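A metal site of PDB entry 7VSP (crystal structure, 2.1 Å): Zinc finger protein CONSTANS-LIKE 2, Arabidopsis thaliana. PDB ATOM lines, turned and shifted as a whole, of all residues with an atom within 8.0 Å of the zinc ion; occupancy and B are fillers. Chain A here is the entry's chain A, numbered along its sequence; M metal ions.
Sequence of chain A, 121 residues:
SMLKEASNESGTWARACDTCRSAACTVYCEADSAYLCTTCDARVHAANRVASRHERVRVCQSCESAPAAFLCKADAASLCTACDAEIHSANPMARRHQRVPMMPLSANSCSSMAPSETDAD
The zinc ion is bound by SG of Cys 80 (2.3 Å), SG of Cys 83 (2.3 Å), SG of Cys 60 (2.4 Å) and SG of Cys 63 (2.4 Å).
The backbone NH of Ala 82 sits close to the side-chain sulfur of Cys 80 (3.8 Å). The side-chain hydroxyl of Ser 62 sits close to the side-chain sulfur of Cys 83, at 3.4 Å. SG of Cys 60 lies close to N of Ser 62 (3.3 Å). The backbone carbonyl oxygen (O) of Ala 66 sits at hydrogen-bond distance from the backbone NH (N) of Cys 60 (2.7 Å). The backbone NH of Ala 66 lies close to the side-chain sulfur of Cys 63, at 3.8 Å. The side-chain sulfur (SG) of Cys 63 sits close to the backbone NH (N) of Ser 65, at 3.4 Å.
Four residues have an atom within 4 Å of the zinc ion: Cys 60, Cys 63, Cys 80 and Cys 83. The nearest printed residue that does not touch the zinc ion is Ser 62 (4.5 Å).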
ATOM      1  N   VAL A  59     -23.876  13.018 -33.050  1.00  0.00           N
ATOM      2  CA  VAL A  59     -23.185  12.520 -31.865  1.00  0.00           C
ATOM      3  C   VAL A  59     -24.152  11.630 -31.075  1.00  0.00           C
ATOM      4  O   VAL A  59     -25.361  11.891 -31.037  1.00  0.00           O
ATOM      5  CB  VAL A  59     -22.661  13.698 -31.023  1.00  0.00           C
ATOM      6  CG1 VAL A  59     -22.250  13.232 -29.605  1.00  0.00           C
ATOM      7  CG2 VAL A  59     -21.478  14.424 -31.726  1.00  0.00           C
ATOM      8  N   CYS A  60     -23.636  10.538 -30.499  1.00  0.00           N
ATOM      9  CA  CYS A  60     -24.419   9.626 -29.672  1.00  0.00           C
ATOM     10  C   CYS A  60     -25.284  10.385 -28.677  1.00  0.00           C
ATOM     11  O   CYS A  60     -24.781  11.178 -27.877  1.00  0.00           O
ATOM     12  CB  CYS A  60     -23.481   8.695 -28.907  1.00  0.00           C
ATOM     13  SG  CYS A  60     -24.332   7.440 -27.894  1.00  0.00           S
ATOM     14  N   GLN A  61     -26.588  10.124 -28.690  1.00  0.00           N
ATOM     15  CA  GLN A  61     -27.484  10.758 -27.729  1.00  0.00           C
ATOM     16  C   GLN A  61     -27.514  10.039 -26.374  1.00  0.00           C
ATOM     17  O   GLN A  61     -28.193  10.494 -25.456  1.00  0.00           O
ATOM     18  CB  GLN A  61     -28.873  10.869 -28.319  1.00  0.00           C
ATOM     19  CG  GLN A  61     -28.885  11.703 -29.628  1.00  0.00           C
ATOM     20  CD  GLN A  61     -30.216  11.613 -30.318  1.00  0.00           C
ATOM     21  OE1 GLN A  61     -30.580  10.574 -30.839  1.00  0.00           O
ATOM     22  NE2 GLN A  61     -30.982  12.694 -30.265  1.00  0.00           N
ATOM     23  N   SER A  62     -26.758   8.965 -26.216  1.00  0.00           N
ATOM     24  CA  SER A  62     -26.625   8.322 -24.912  1.00  0.00           C
ATOM     25  C   SER A  62     -25.436   8.913 -24.159  1.00  0.00           C
ATOM     26  O   SER A  62     -25.621   9.590 -23.144  1.00  0.00           O
ATOM     27  CB  SER A  62     -26.493   6.798 -25.105  1.00  0.00           C
ATOM     28  OG  SER A  62     -26.127   6.140 -23.900  1.00  0.00           O
ATOM     29  N   CYS A  63     -24.221   8.720 -24.664  1.00  0.00           N
ATOM     30  CA  CYS A  63     -23.040   9.244 -23.978  1.00  0.00           C
ATOM     31  C   CYS A  63     -22.709  10.673 -24.387  1.00  0.00           C
ATOM     32  O   CYS A  63     -21.917  11.322 -23.693  1.00  0.00           O
ATOM     33  CB  CYS A  63     -21.823   8.339 -24.235  1.00  0.00           C
ATOM     34  SG  CYS A  63     -21.176   8.375 -26.010  1.00  0.00           S
ATOM     35  N   GLU A  64     -23.116  11.044 -25.600  1.00  0.00           N
ATOM     36  CA  GLU A  64     -22.933  12.413 -26.148  1.00  0.00           C
ATOM     37  C   GLU A  64     -21.438  12.711 -26.322  1.00  0.00           C
ATOM     38  O   GLU A  64     -21.102  13.904 -26.491  1.00  0.00           O
ATOM     39  CB  GLU A  64     -23.606  13.452 -25.240  1.00  0.00           C
ATOM     40  CG  GLU A  64     -25.124  13.418 -25.304  1.00  0.00           C
ATOM     41  CD  GLU A  64     -25.823  14.082 -24.133  1.00  0.00           C
ATOM     42  OE1 GLU A  64     -25.166  14.878 -23.435  1.00  0.00           O
ATOM     43  OE2 GLU A  64     -27.014  13.802 -23.921  1.00  0.00           O
ATOM     44  N   SER A  65     -20.595  11.684 -26.278  1.00  0.00           N
ATOM     45  CA  SER A  65     -19.127  11.893 -26.399  1.00  0.00           C
ATOM     46  C   SER A  65     -18.531  11.073 -27.557  1.00  0.00           C
ATOM     47  O   SER A  65     -17.293  10.919 -27.574  1.00  0.00           O
ATOM     48  CB  SER A  65     -18.434  11.587 -25.095  1.00  0.00           C
ATOM     49  OG  SER A  65     -17.140  12.173 -25.063  1.00  0.00           O
ATOM     50  N   ALA A  66     -19.353  10.569 -28.477  1.00  0.00           N
ATOM     51  CA  ALA A  66     -18.800   9.738 -29.549  1.00  0.00           C
ATOM     52  C   ALA A  66     -19.736   9.847 -30.733  1.00  0.00           C
ATOM     53  O   ALA A  66     -20.915  10.153 -30.560  1.00  0.00           O
ATOM     54  CB  ALA A  66     -18.635   8.268 -29.107  1.00  0.00           C
ATOM     55  N   PRO A  67     -19.244   9.591 -31.957  1.00  0.00           N
ATOM     56  CA  PRO A  67     -20.162   9.628 -33.104  1.00  0.00           C
ATOM     57  C   PRO A  67     -21.146   8.484 -33.021  1.00  0.00           C
ATOM     58  O   PRO A  67     -20.792   7.390 -32.600  1.00  0.00           O
ATOM     59  CB  PRO A  67     -19.228   9.459 -34.326  1.00  0.00           C
ATOM     60  CG  PRO A  67     -17.856   9.285 -33.815  1.00  0.00           C
ATOM     61  CD  PRO A  67     -17.887   9.129 -32.331  1.00  0.00           C
ATOM     62  N   ALA A  68     -22.380   8.740 -33.416  1.00  0.00           N
ATOM     63  CA  ALA A  68     -23.373   7.675 -33.515  1.00  0.00           C
ATOM     64  C   ALA A  68     -23.093   6.766 -34.726  1.00  0.00           C
ATOM     65  O   ALA A  68     -22.635   7.210 -35.767  1.00  0.00           O
ATOM     66  CB  ALA A  68     -24.773   8.279 -33.656  1.00  0.00           C
ATOM     67  N   ALA A  69     -23.418   5.485 -34.582  1.00  0.00           N
ATOM     68  CA  ALA A  69     -23.312   4.525 -35.666  1.00  0.00           C
ATOM     69  C   ALA A  69     -24.601   3.762 -35.939  1.00  0.00           C
ATOM     70  O   ALA A  69     -24.723   3.171 -37.030  1.00  0.00           O
ATOM     71  CB  ALA A  69     -22.183   3.520 -35.368  1.00  0.00           C
ATOM     72  N   SER A  78     -29.991   7.992 -31.766  1.00  0.00           N
ATOM     73  CA  SER A  78     -28.771   7.623 -32.450  1.00  0.00           C
ATOM     74  C   SER A  78     -27.682   7.313 -31.430  1.00  0.00           C
ATOM     75  O   SER A  78     -27.407   8.137 -30.556  1.00  0.00           O
ATOM     76  CB  SER A  78     -28.341   8.764 -33.383  1.00  0.00           C
ATOM     77  OG  SER A  78     -29.435   9.155 -34.190  1.00  0.00           O
ATOM     78  N   LEU A  79     -27.086   6.120 -31.544  1.00  0.00           N
ATOM     79  CA  LEU A  79     -26.149   5.613 -30.553  1.00  0.00           C
ATOM     80  C   LEU A  79     -24.801   5.230 -31.169  1.00  0.00           C
ATOM     81  O   LEU A  79     -24.743   4.631 -32.242  1.00  0.00           O
ATOM     82  CB  LEU A  79     -26.736   4.397 -29.845  1.00  0.00           C
ATOM     83  CG  LEU A  79     -28.156   4.546 -29.304  1.00  0.00           C
ATOM     84  CD1 LEU A  79     -28.770   3.160 -28.929  1.00  0.00           C
ATOM     85  CD2 LEU A  79     -28.094   5.504 -28.115  1.00  0.00           C
ATOM     86  N   CYS A  80     -23.725   5.523 -30.449  1.00  0.00           N
ATOM     87  CA  CYS A  80     -22.423   5.016 -30.835  1.00  0.00           C
ATOM     88  C   CYS A  80     -22.390   3.478 -30.693  1.00  0.00           C
ATOM     89  O   CYS A  80     -23.318   2.853 -30.157  1.00  0.00           O
ATOM     90  CB  CYS A  80     -21.321   5.687 -30.008  1.00  0.00           C
ATOM     91  SG  CYS A  80     -21.228   5.176 -28.259  1.00  0.00           S
ATOM     92  N   THR A  81     -21.298   2.864 -31.165  1.00  0.00           N
ATOM     93  CA  THR A  81     -21.224   1.395 -31.144  1.00  0.00           C
ATOM     94  C   THR A  81     -21.314   0.864 -29.718  1.00  0.00           C
ATOM     95  O   THR A  81     -22.093  -0.062 -29.442  1.00  0.00           O
ATOM     96  CB  THR A  81     -19.933   0.904 -31.808  1.00  0.00           C
ATOM     97  OG1 THR A  81     -19.937   1.332 -33.158  1.00  0.00           O
ATOM     98  CG2 THR A  81     -19.890  -0.622 -31.827  1.00  0.00           C
ATOM     99  N   ALA A  82     -20.551   1.478 -28.804  1.00  0.00           N
ATOM    100  CA  ALA A  82     -20.506   1.011 -27.422  1.00  0.00           C
ATOM    101  C   ALA A  82     -21.835   1.241 -26.707  1.00  0.00           C
ATOM    102  O   ALA A  82     -22.311   0.355 -25.973  1.00  0.00           O
ATOM    103  CB  ALA A  82     -19.364   1.720 -26.671  1.00  0.00           C
ATOM    104  N   CYS A  83     -22.452   2.415 -26.884  1.00  0.00           N
ATOM    105  CA  CYS A  83     -23.762   2.634 -26.282  1.00  0.00           C
ATOM    106  C   CYS A  83     -24.828   1.731 -26.896  1.00  0.00           C
ATOM    107  O   CYS A  83     -25.738   1.266 -26.191  1.00  0.00           O
ATOM    108  CB  CYS A  83     -24.162   4.116 -26.387  1.00  0.00           C
ATOM    109  SG  CYS A  83     -23.193   5.127 -25.192  1.00  0.00           S
ATOM    110  N   ASP A  84     -24.732   1.476 -28.206  1.00  0.00           N
ATOM    111  CA  ASP A  84     -25.682   0.576 -28.845  1.00  0.00           C
ATOM    112  C   ASP A  84     -25.614  -0.821 -28.245  1.00  0.00           C
ATOM    113  O   ASP A  84     -26.634  -1.482 -28.070  1.00  0.00           O
ATOM    114  CB  ASP A  84     -25.447   0.489 -30.364  1.00  0.00           C
ATOM    115  CG  ASP A  84     -26.412  -0.467 -31.036  1.00  0.00           C
ATOM    116  OD1 ASP A  84     -27.629  -0.165 -31.094  1.00  0.00           O
ATOM    117  OD2 ASP A  84     -25.967  -1.536 -31.511  1.00  0.00           O
ATOM    118  N   GLU A  86     -24.361  -1.564 -25.132  1.00  0.00           N
ATOM    119  CA  GLU A  86     -24.742  -1.537 -23.727  1.00  0.00           C
ATOM    120  C   GLU A  86     -26.258  -1.475 -23.578  1.00  0.00           C
ATOM    121  O   GLU A  86     -26.845  -2.212 -22.778  1.00  0.00           O
ATOM    122  CB  GLU A  86     -24.115  -0.345 -23.010  1.00  0.00           C
ATOM    123  CG  GLU A  86     -24.685  -0.089 -21.593  1.00  0.00           C
ATOM    124  CD  GLU A  86     -24.445   1.334 -21.057  1.00  0.00           C
ATOM    125  OE1 GLU A  86     -23.276   1.656 -20.776  1.00  0.00           O
ATOM    126  OE2 GLU A  86     -25.420   2.106 -20.879  1.00  0.00           O
ATOM    127  N   ILE A  87     -26.897  -0.608 -24.352  1.00  0.00           N
ATOM    128  CA  ILE A  87     -28.337  -0.403 -24.185  1.00  0.00           C
ATOM    129  C   ILE A  87     -29.128  -1.637 -24.611  1.00  0.00           C
ATOM    130  O   ILE A  87     -30.081  -2.037 -23.927  1.00  0.00           O
ATOM    131  CB  ILE A  87     -28.761   0.867 -24.945  1.00  0.00           C
ATOM    132  CG1 ILE A  87     -28.362   2.097 -24.109  1.00  0.00           C
ATOM    133  CG2 ILE A  87     -30.254   0.837 -25.332  1.00  0.00           C
ATOM    134  CD1 ILE A  87     -28.482   3.390 -24.846  1.00  0.00           C
HETATM  135 ZN    ZN M   1     -22.399   6.498 -26.860  1.00  0.00          ZN
